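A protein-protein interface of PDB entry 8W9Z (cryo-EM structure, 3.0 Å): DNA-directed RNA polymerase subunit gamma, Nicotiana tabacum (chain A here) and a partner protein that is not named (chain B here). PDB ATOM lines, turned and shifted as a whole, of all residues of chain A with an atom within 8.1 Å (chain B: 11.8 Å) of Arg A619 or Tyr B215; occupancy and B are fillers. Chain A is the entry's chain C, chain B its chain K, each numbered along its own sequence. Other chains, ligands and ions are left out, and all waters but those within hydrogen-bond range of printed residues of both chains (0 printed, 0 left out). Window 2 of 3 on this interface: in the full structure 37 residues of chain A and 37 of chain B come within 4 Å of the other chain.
Arg A619 touches just one residue of chain B: Tyr B215. Tyr B215 touches just one residue of chain A: Arg A619. Of chain B, only Val B202 (3.5 Å) comes within 4 Å of Val A620. Ile A621 touches one residue of chain B. Of the printed residues of chain A, Ser B217 touches Gln A618 (3.8 Å). Of the printed residues of chain B, Ala A622 touches Val B202. Asn B201 touches none of the printed residues of chain A. The nearest printed residue of chain B that does not touch Arg A619 is Val B202 (5.1 Å). The nearest residue of chain A that does not touch Tyr B215 is Ile A621 (5.1 Å). The nearest printed residue of chain A that does not touch Val B202 is Arg A619 (5.1 Å).
Hydrophobic or aromatic side chains of chain B that line the printed part of chain A: Val B202 and Tyr B215. Along chain A the printed residues that touch a printed residue of chain B span positions 618 to 622. Among the printed residues, no Asp or Glu carboxylate lies within 4 Å of a Lys or Arg side-chain nitrogen of the other chain.
Among the printed residues, pairs that only touch across the chains: Gln A618 with Ser B217, Arg A619 with Tyr B215, Val A620 with Val B202, Ile A621 with Val B202 and Ala A622 with Val B202.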
ATOM      1  N   TRP A 614      -7.804 -24.000 -22.506  1.00  0.00           N
ATOM      2  CA  TRP A 614      -8.814 -22.962 -22.653  1.00  0.00           C
ATOM      3  C   TRP A 614      -8.751 -22.402 -24.066  1.00  0.00           C
ATOM      4  O   TRP A 614      -7.665 -22.099 -24.571  1.00  0.00           O
ATOM      5  CB  TRP A 614      -8.607 -21.853 -21.622  1.00  0.00           C
ATOM      6  N   ARG A 615      -9.916 -22.261 -24.700  1.00  0.00           N
ATOM      7  CA  ARG A 615      -9.993 -21.900 -26.115  1.00  0.00           C
ATOM      8  C   ARG A 615      -9.874 -20.385 -26.307  1.00  0.00           C
ATOM      9  O   ARG A 615     -10.706 -19.740 -26.944  1.00  0.00           O
ATOM     10  CB  ARG A 615     -11.283 -22.437 -26.721  1.00  0.00           C
ATOM     11  N   LEU A 616      -8.793 -19.837 -25.748  1.00  0.00           N
ATOM     12  CA  LEU A 616      -8.413 -18.424 -25.873  1.00  0.00           C
ATOM     13  C   LEU A 616      -9.621 -17.491 -25.791  1.00  0.00           C
ATOM     14  O   LEU A 616      -9.810 -16.593 -26.614  1.00  0.00           O
ATOM     15  CB  LEU A 616      -7.612 -18.176 -27.157  1.00  0.00           C
ATOM     16  N   ASP A 617     -10.446 -17.710 -24.767  1.00  0.00           N
ATOM     17  CA  ASP A 617     -11.609 -16.856 -24.552  1.00  0.00           C
ATOM     18  C   ASP A 617     -11.236 -15.479 -24.018  1.00  0.00           C
ATOM     19  O   ASP A 617     -12.101 -14.598 -23.976  1.00  0.00           O
ATOM     20  CB  ASP A 617     -12.591 -17.535 -23.598  1.00  0.00           C
ATOM     21  CG  ASP A 617     -13.064 -18.881 -24.110  1.00  0.00           C
ATOM     22  OD1 ASP A 617     -13.072 -19.080 -25.342  1.00  0.00           O
ATOM     23  OD2 ASP A 617     -13.429 -19.740 -23.279  1.00  0.00           O
ATOM     24  N   GLN A 618      -9.986 -15.284 -23.598  1.00  0.00           N
ATOM     25  CA  GLN A 618      -9.438 -14.010 -23.140  1.00  0.00           C
ATOM     26  C   GLN A 618     -10.105 -13.494 -21.867  1.00  0.00           C
ATOM     27  O   GLN A 618      -9.773 -12.398 -21.401  1.00  0.00           O
ATOM     28  CB  GLN A 618      -9.509 -12.942 -24.241  1.00  0.00           C
ATOM     29  CG  GLN A 618      -8.414 -11.887 -24.169  1.00  0.00           C
ATOM     30  CD  GLN A 618      -8.475 -10.902 -25.320  1.00  0.00           C
ATOM     31  OE1 GLN A 618      -9.351 -10.989 -26.181  1.00  0.00           O
ATOM     32  NE2 GLN A 618      -7.542  -9.957 -25.341  1.00  0.00           N
ATOM     33  N   ARG A 619     -11.029 -14.251 -21.288  1.00  0.00           N
ATOM     34  CA  ARG A 619     -11.654 -13.880 -20.019  1.00  0.00           C
ATOM     35  C   ARG A 619     -10.927 -14.552 -18.856  1.00  0.00           C
ATOM     36  O   ARG A 619     -11.510 -15.269 -18.043  1.00  0.00           O
ATOM     37  CB  ARG A 619     -13.137 -14.243 -20.034  1.00  0.00           C
ATOM     38  N   VAL A 620      -9.622 -14.299 -18.789  1.00  0.00           N
ATOM     39  CA  VAL A 620      -8.757 -14.941 -17.807  1.00  0.00           C
ATOM     40  C   VAL A 620      -9.009 -14.337 -16.433  1.00  0.00           C
ATOM     41  O   VAL A 620      -8.565 -13.220 -16.142  1.00  0.00           O
ATOM     42  CB  VAL A 620      -7.276 -14.815 -18.203  1.00  0.00           C
ATOM     43  CG1 VAL A 620      -6.422 -15.714 -17.332  1.00  0.00           C
ATOM     44  CG2 VAL A 620      -7.090 -15.150 -19.674  1.00  0.00           C
ATOM     45  N   ILE A 621      -9.716 -15.072 -15.581  1.00  0.00           N
ATOM     46  CA  ILE A 621     -10.065 -14.585 -14.251  1.00  0.00           C
ATOM     47  C   ILE A 621      -8.889 -14.830 -13.314  1.00  0.00           C
ATOM     48  O   ILE A 621      -8.473 -15.975 -13.110  1.00  0.00           O
ATOM     49  CB  ILE A 621     -11.338 -15.265 -13.729  1.00  0.00           C
ATOM     50  CG1 ILE A 621     -12.466 -15.143 -14.756  1.00  0.00           C
ATOM     51  CG2 ILE A 621     -11.756 -14.660 -12.398  1.00  0.00           C
ATOM     52  CD1 ILE A 621     -12.783 -13.717 -15.152  1.00  0.00           C
ATOM     53  N   ALA A 622      -8.357 -13.756 -12.741  1.00  0.00           N
ATOM     54  CA  ALA A 622      -7.231 -13.841 -11.818  1.00  0.00           C
ATOM     55  C   ALA A 622      -7.183 -12.552 -11.006  1.00  0.00           C
ATOM     56  O   ALA A 622      -8.109 -11.735 -11.048  1.00  0.00           O
ATOM     57  CB  ALA A 622      -5.921 -14.092 -12.571  1.00  0.00           C
ATOM     58  N   ILE A 658      -3.553 -21.358 -24.138  1.00  0.00           N
ATOM     59  CA  ILE A 658      -3.897 -20.965 -22.776  1.00  0.00           C
ATOM     60  C   ILE A 658      -4.341 -22.214 -22.030  1.00  0.00           C
ATOM     61  O   ILE A 658      -5.266 -22.907 -22.470  1.00  0.00           O
ATOM     62  CB  ILE A 658      -4.998 -19.894 -22.733  1.00  0.00           C
ATOM     63  CG1 ILE A 658      -4.485 -18.568 -23.291  1.00  0.00           C
ATOM     64  CG2 ILE A 658      -5.499 -19.705 -21.311  1.00  0.00           C
ATOM     65  CD1 ILE A 658      -5.492 -17.444 -23.203  1.00  0.00           C
ATOM     66  N   ILE A 660      -5.422 -23.751 -18.092  1.00  0.00           N
ATOM     67  CA  ILE A 660      -5.925 -23.380 -16.777  1.00  0.00           C
ATOM     68  C   ILE A 660      -5.685 -24.545 -15.828  1.00  0.00           C
ATOM     69  O   ILE A 660      -5.968 -25.700 -16.170  1.00  0.00           O
ATOM     70  CB  ILE A 660      -7.419 -23.016 -16.827  1.00  0.00           C
ATOM     71  CG1 ILE A 660      -7.701 -22.057 -17.985  1.00  0.00           C
ATOM     72  CG2 ILE A 660      -7.860 -22.397 -15.513  1.00  0.00           C
ATOM     73  CD1 ILE A 660      -7.020 -20.716 -17.850  1.00  0.00           C
ATOM     74  N   TYR A 670     -19.154 -24.662 -13.898  1.00  0.00           N
ATOM     75  CA  TYR A 670     -19.193 -23.790 -15.067  1.00  0.00           C
ATOM     76  C   TYR A 670     -19.930 -24.458 -16.222  1.00  0.00           C
ATOM     77  O   TYR A 670     -20.776 -23.837 -16.879  1.00  0.00           O
ATOM     78  CB  TYR A 670     -17.772 -23.405 -15.477  1.00  0.00           C
ATOM     79  CG  TYR A 670     -17.700 -22.499 -16.686  1.00  0.00           C
ATOM     80  CD1 TYR A 670     -17.882 -21.129 -16.561  1.00  0.00           C
ATOM     81  CD2 TYR A 670     -17.444 -23.013 -17.950  1.00  0.00           C
ATOM     82  CE1 TYR A 670     -17.816 -20.295 -17.661  1.00  0.00           C
ATOM     83  CE2 TYR A 670     -17.377 -22.189 -19.056  1.00  0.00           C
ATOM     84  CZ  TYR A 670     -17.564 -20.832 -18.906  1.00  0.00           C
ATOM     85  OH  TYR A 670     -17.497 -20.005 -20.004  1.00  0.00           O
ATOM     86  N   CYS B 199      -0.349  -7.976 -15.658  1.00  0.00           N
ATOM     87  CA  CYS B 199      -1.281  -8.910 -15.041  1.00  0.00           C
ATOM     88  C   CYS B 199      -2.703  -8.449 -15.313  1.00  0.00           C
ATOM     89  O   CYS B 199      -3.022  -7.271 -15.124  1.00  0.00           O
ATOM     90  CB  CYS B 199      -1.032  -9.021 -13.532  1.00  0.00           C
ATOM     91  SG  CYS B 199      -1.026  -7.445 -12.650  1.00  0.00           S
ATOM     92  N   TYR B 200      -3.547  -9.376 -15.757  1.00  0.00           N
ATOM     93  CA  TYR B 200      -4.934  -9.050 -16.053  1.00  0.00           C
ATOM     94  C   TYR B 200      -5.675  -8.652 -14.782  1.00  0.00           C
ATOM     95  O   TYR B 200      -5.395  -9.150 -13.688  1.00  0.00           O
ATOM     96  CB  TYR B 200      -5.632 -10.237 -16.715  1.00  0.00           C
ATOM     97  CG  TYR B 200      -5.038 -10.639 -18.044  1.00  0.00           C
ATOM     98  CD1 TYR B 200      -3.993 -11.551 -18.113  1.00  0.00           C
ATOM     99  CD2 TYR B 200      -5.524 -10.111 -19.232  1.00  0.00           C
ATOM    100  CE1 TYR B 200      -3.449 -11.923 -19.325  1.00  0.00           C
ATOM    101  CE2 TYR B 200      -4.986 -10.477 -20.449  1.00  0.00           C
ATOM    102  CZ  TYR B 200      -3.948 -11.383 -20.489  1.00  0.00           C
ATOM    103  OH  TYR B 200      -3.408 -11.751 -21.699  1.00  0.00           O
ATOM    104  N   ASN B 201      -6.634  -7.742 -14.937  1.00  0.00           N
ATOM    105  CA  ASN B 201      -7.446  -7.247 -13.827  1.00  0.00           C
ATOM    106  C   ASN B 201      -8.913  -7.401 -14.211  1.00  0.00           C
ATOM    107  O   ASN B 201      -9.454  -6.583 -14.961  1.00  0.00           O
ATOM    108  CB  ASN B 201      -7.108  -5.797 -13.502  1.00  0.00           C
ATOM    109  CG  ASN B 201      -7.932  -5.250 -12.355  1.00  0.00           C
ATOM    110  OD1 ASN B 201      -8.397  -5.999 -11.497  1.00  0.00           O
ATOM    111  ND2 ASN B 201      -8.122  -3.936 -12.336  1.00  0.00           N
ATOM    112  N   VAL B 202      -9.555  -8.445 -13.697  1.00  0.00           N
ATOM    113  CA  VAL B 202     -10.963  -8.712 -13.962  1.00  0.00           C
ATOM    114  C   VAL B 202     -11.779  -8.170 -12.796  1.00  0.00           C
ATOM    115  O   VAL B 202     -11.572  -8.565 -11.641  1.00  0.00           O
ATOM    116  CB  VAL B 202     -11.223 -10.212 -14.180  1.00  0.00           C
ATOM    117  CG1 VAL B 202     -10.818 -10.613 -15.588  1.00  0.00           C
ATOM    118  CG2 VAL B 202     -10.465 -11.043 -13.160  1.00  0.00           C
ATOM    119  N   THR B 203     -12.695  -7.257 -13.095  1.00  0.00           N
ATOM    120  CA  THR B 203     -13.535  -6.624 -12.093  1.00  0.00           C
ATOM    121  C   THR B 203     -14.998  -6.942 -12.366  1.00  0.00           C
ATOM    122  O   THR B 203     -15.373  -7.355 -13.467  1.00  0.00           O
ATOM    123  CB  THR B 203     -13.327  -5.105 -12.067  1.00  0.00           C
ATOM    124  OG1 THR B 203     -14.221  -4.513 -11.116  1.00  0.00           O
ATOM    125  CG2 THR B 203     -13.588  -4.507 -13.441  1.00  0.00           C
ATOM    126  N   GLU B 204     -15.827  -6.748 -11.339  1.00  0.00           N
ATOM    127  CA  GLU B 204     -17.257  -6.997 -11.440  1.00  0.00           C
ATOM    128  C   GLU B 204     -17.985  -5.663 -11.536  1.00  0.00           C
ATOM    129  O   GLU B 204     -18.232  -5.023 -10.503  1.00  0.00           O
ATOM    130  CB  GLU B 204     -17.751  -7.798 -10.232  1.00  0.00           C
ATOM    131  CG  GLU B 204     -16.961  -9.072  -9.962  1.00  0.00           C
ATOM    132  CD  GLU B 204     -17.070 -10.087 -11.085  1.00  0.00           C
ATOM    133  OE1 GLU B 204     -18.074 -10.056 -11.829  1.00  0.00           O
ATOM    134  OE2 GLU B 204     -16.148 -10.918 -11.226  1.00  0.00           O
ATOM    135  N   PRO B 205     -18.347  -5.203 -12.728  1.00  0.00           N
ATOM    136  CA  PRO B 205     -18.963  -3.884 -12.860  1.00  0.00           C
ATOM    137  C   PRO B 205     -20.423  -3.918 -12.451  1.00  0.00           C
ATOM    138  O   PRO B 205     -21.058  -4.984 -12.465  1.00  0.00           O
ATOM    139  CB  PRO B 205     -18.811  -3.579 -14.356  1.00  0.00           C
ATOM    140  CG  PRO B 205     -18.848  -4.918 -14.997  1.00  0.00           C
ATOM    141  CD  PRO B 205     -18.172  -5.864 -14.033  1.00  0.00           C
ATOM    142  N   PRO B 206     -20.989  -2.775 -12.071  1.00  0.00           N
ATOM    143  CA  PRO B 206     -22.415  -2.734 -11.738  1.00  0.00           C
ATOM    144  C   PRO B 206     -23.279  -3.001 -12.959  1.00  0.00           C
ATOM    145  O   PRO B 206     -22.929  -2.652 -14.089  1.00  0.00           O
ATOM    146  CB  PRO B 206     -22.619  -1.305 -11.218  1.00  0.00           C
ATOM    147  CG  PRO B 206     -21.252  -0.837 -10.835  1.00  0.00           C
ATOM    148  CD  PRO B 206     -20.322  -1.492 -11.803  1.00  0.00           C
ATOM    149  N   ILE B 207     -24.425  -3.629 -12.716  1.00  0.00           N
ATOM    150  CA  ILE B 207     -25.366  -3.999 -13.768  1.00  0.00           C
ATOM    151  C   ILE B 207     -26.588  -3.101 -13.638  1.00  0.00           C
ATOM    152  O   ILE B 207     -27.403  -3.269 -12.723  1.00  0.00           O
ATOM    153  CB  ILE B 207     -25.755  -5.481 -13.690  1.00  0.00           C
ATOM    154  CG1 ILE B 207     -24.515  -6.366 -13.829  1.00  0.00           C
ATOM    155  CG2 ILE B 207     -26.775  -5.820 -14.763  1.00  0.00           C
ATOM    156  CD1 ILE B 207     -24.813  -7.845 -13.759  1.00  0.00           C
ATOM    157  N   ASP B 208     -26.718  -2.144 -14.555  1.00  0.00           N
ATOM    158  CA  ASP B 208     -27.861  -1.240 -14.622  1.00  0.00           C
ATOM    159  C   ASP B 208     -28.475  -1.267 -16.012  1.00  0.00           C
ATOM    160  O   ASP B 208     -28.851  -0.233 -16.571  1.00  0.00           O
ATOM    161  CB  ASP B 208     -27.462   0.180 -14.233  1.00  0.00           C
ATOM    162  CG  ASP B 208     -27.370   0.368 -12.734  1.00  0.00           C
ATOM    163  OD1 ASP B 208     -27.850  -0.517 -11.995  1.00  0.00           O
ATOM    164  OD2 ASP B 208     -26.818   1.398 -12.293  1.00  0.00           O
ATOM    165  N   ALA B 209     -28.585  -2.459 -16.590  1.00  0.00           N
ATOM    166  CA  ALA B 209     -29.100  -2.635 -17.938  1.00  0.00           C
ATOM    167  C   ALA B 209     -29.617  -4.060 -18.067  1.00  0.00           C
ATOM    168  O   ALA B 209     -29.193  -4.945 -17.314  1.00  0.00           O
ATOM    169  CB  ALA B 209     -28.014  -2.352 -18.989  1.00  0.00           C
ATOM    170  N   ARG B 211     -28.949  -6.220 -20.335  1.00  0.00           N
ATOM    171  CA  ARG B 211     -27.898  -7.108 -20.821  1.00  0.00           C
ATOM    172  C   ARG B 211     -26.525  -6.497 -20.571  1.00  0.00           C
ATOM    173  O   ARG B 211     -25.636  -6.549 -21.427  1.00  0.00           O
ATOM    174  CB  ARG B 211     -28.091  -7.431 -22.301  1.00  0.00           C
ATOM    175  CG  ARG B 211     -28.185  -6.212 -23.203  1.00  0.00           C
ATOM    176  CD  ARG B 211     -28.635  -6.603 -24.597  1.00  0.00           C
ATOM    177  NE  ARG B 211     -29.963  -7.205 -24.579  1.00  0.00           N
ATOM    178  CZ  ARG B 211     -31.094  -6.510 -24.616  1.00  0.00           C
ATOM    179  NH1 ARG B 211     -31.055  -5.186 -24.677  1.00  0.00           N
ATOM    180  NH2 ARG B 211     -32.262  -7.135 -24.594  1.00  0.00           N
ATOM    181  N   ASP B 212     -26.332  -5.918 -19.391  1.00  0.00           N
ATOM    182  CA  ASP B 212     -25.048  -5.321 -19.060  1.00  0.00           C
ATOM    183  C   ASP B 212     -23.989  -6.410 -18.899  1.00  0.00           C
ATOM    184  O   ASP B 212     -24.279  -7.484 -18.364  1.00  0.00           O
ATOM    185  CB  ASP B 212     -25.158  -4.502 -17.774  1.00  0.00           C
ATOM    186  CG  ASP B 212     -23.856  -3.819 -17.403  1.00  0.00           C
ATOM    187  OD1 ASP B 212     -23.509  -2.807 -18.049  1.00  0.00           O
ATOM    188  OD2 ASP B 212     -23.180  -4.294 -16.466  1.00  0.00           O
ATOM    189  N   PRO B 213     -22.764  -6.172 -19.368  1.00  0.00           N
ATOM    190  CA  PRO B 213     -21.708  -7.180 -19.212  1.00  0.00           C
ATOM    191  C   PRO B 213     -21.431  -7.472 -17.745  1.00  0.00           C
ATOM    192  O   PRO B 213     -21.337  -6.564 -16.916  1.00  0.00           O
ATOM    193  CB  PRO B 213     -20.498  -6.534 -19.895  1.00  0.00           C
ATOM    194  CG  PRO B 213     -21.087  -5.559 -20.858  1.00  0.00           C
ATOM    195  CD  PRO B 213     -22.323  -5.034 -20.191  1.00  0.00           C
ATOM    196  N   MET B 214     -21.300  -8.761 -17.429  1.00  0.00           N
ATOM    197  CA  MET B 214     -21.102  -9.183 -16.049  1.00  0.00           C
ATOM    198  C   MET B 214     -19.665  -9.012 -15.574  1.00  0.00           C
ATOM    199  O   MET B 214     -19.435  -8.936 -14.362  1.00  0.00           O
ATOM    200  CB  MET B 214     -21.528 -10.642 -15.878  1.00  0.00           C
ATOM    201  CG  MET B 214     -22.979 -10.908 -16.235  1.00  0.00           C
ATOM    202  SD  MET B 214     -23.507 -12.571 -15.785  1.00  0.00           S
ATOM    203  CE  MET B 214     -23.271 -12.525 -14.011  1.00  0.00           C
ATOM    204  N   TYR B 215     -18.698  -8.956 -16.487  1.00  0.00           N
ATOM    205  CA  TYR B 215     -17.300  -8.811 -16.112  1.00  0.00           C
ATOM    206  C   TYR B 215     -16.614  -7.842 -17.064  1.00  0.00           C
ATOM    207  O   TYR B 215     -17.109  -7.551 -18.154  1.00  0.00           O
ATOM    208  CB  TYR B 215     -16.571 -10.162 -16.115  1.00  0.00           C
ATOM    209  CG  TYR B 215     -16.484 -10.816 -17.474  1.00  0.00           C
ATOM    210  CD1 TYR B 215     -17.531 -11.585 -17.965  1.00  0.00           C
ATOM    211  CD2 TYR B 215     -15.352 -10.671 -18.266  1.00  0.00           C
ATOM    212  CE1 TYR B 215     -17.455 -12.186 -19.208  1.00  0.00           C
ATOM    213  CE2 TYR B 215     -15.267 -11.269 -19.509  1.00  0.00           C
ATOM    214  CZ  TYR B 215     -16.321 -12.025 -19.974  1.00  0.00           C
ATOM    215  OH  TYR B 215     -16.241 -12.621 -21.211  1.00  0.00           O
ATOM    216  N   LYS B 216     -15.459  -7.344 -16.629  1.00  0.00           N
ATOM    217  CA  LYS B 216     -14.641  -6.440 -17.425  1.00  0.00           C
ATOM    218  C   LYS B 216     -13.190  -6.879 -17.319  1.00  0.00           C
ATOM    219  O   LYS B 216     -12.701  -7.145 -16.218  1.00  0.00           O
ATOM    220  CB  LYS B 216     -14.798  -4.990 -16.954  1.00  0.00           C
ATOM    221  CG  LYS B 216     -13.983  -3.984 -17.747  1.00  0.00           C
ATOM    222  CD  LYS B 216     -14.192  -2.574 -17.220  1.00  0.00           C
ATOM    223  CE  LYS B 216     -13.379  -1.561 -18.010  1.00  0.00           C
ATOM    224  NZ  LYS B 216     -13.571  -0.175 -17.501  1.00  0.00           N
ATOM    225  N   SER B 217     -12.506  -6.954 -18.458  1.00  0.00           N
ATOM    226  CA  SER B 217     -11.136  -7.440 -18.521  1.00  0.00           C
ATOM    227  C   SER B 217     -10.212  -6.347 -19.039  1.00  0.00           C
ATOM    228  O   SER B 217     -10.532  -5.658 -20.013  1.00  0.00           O
ATOM    229  CB  SER B 217     -11.031  -8.677 -19.418  1.00  0.00           C
ATOM    230  OG  SER B 217      -9.699  -9.154 -19.474  1.00  0.00           O
ATOM    231  N   GLU B 218      -9.065  -6.195 -18.381  1.00  0.00           N
ATOM    232  CA  GLU B 218      -8.047  -5.233 -18.776  1.00  0.00           C
ATOM    233  C   GLU B 218      -6.679  -5.892 -18.680  1.00  0.00           C
ATOM    234  O   GLU B 218      -6.436  -6.702 -17.781  1.00  0.00           O
ATOM    235  CB  GLU B 218      -8.086  -3.976 -17.897  1.00  0.00           C
ATOM    236  CG  GLU B 218      -9.360  -3.156 -18.028  1.00  0.00           C
ATOM    237  CD  GLU B 218      -9.483  -2.474 -19.378  1.00  0.00           C
ATOM    238  OE1 GLU B 218      -8.449  -2.296 -20.056  1.00  0.00           O
ATOM    239  OE2 GLU B 218     -10.615  -2.115 -19.763  1.00  0.00           O
ATOM    240  N   ARG B 219      -5.788  -5.544 -19.611  1.00  0.00           N
ATOM    241  CA  ARG B 219      -4.459  -6.146 -19.616  1.00  0.00           C
ATOM    242  C   ARG B 219      -3.569  -5.545 -18.534  1.00  0.00           C
ATOM    243  O   ARG B 219      -2.903  -6.276 -17.793  1.00  0.00           O
ATOM    244  CB  ARG B 219      -3.812  -5.991 -20.992  1.00  0.00           C
ATOM    245  CG  ARG B 219      -2.415  -6.579 -21.075  1.00  0.00           C
ATOM    246  CD  ARG B 219      -2.408  -8.036 -20.643  1.00  0.00           C
ATOM    247  NE  ARG B 219      -1.056  -8.531 -20.400  1.00  0.00           N
ATOM    248  CZ  ARG B 219      -0.297  -9.113 -21.322  1.00  0.00           C
ATOM    249  NH1 ARG B 219      -0.755  -9.276 -22.555  1.00  0.00           N
ATOM    250  NH2 ARG B 219       0.922  -9.532 -21.011  1.00  0.00           N
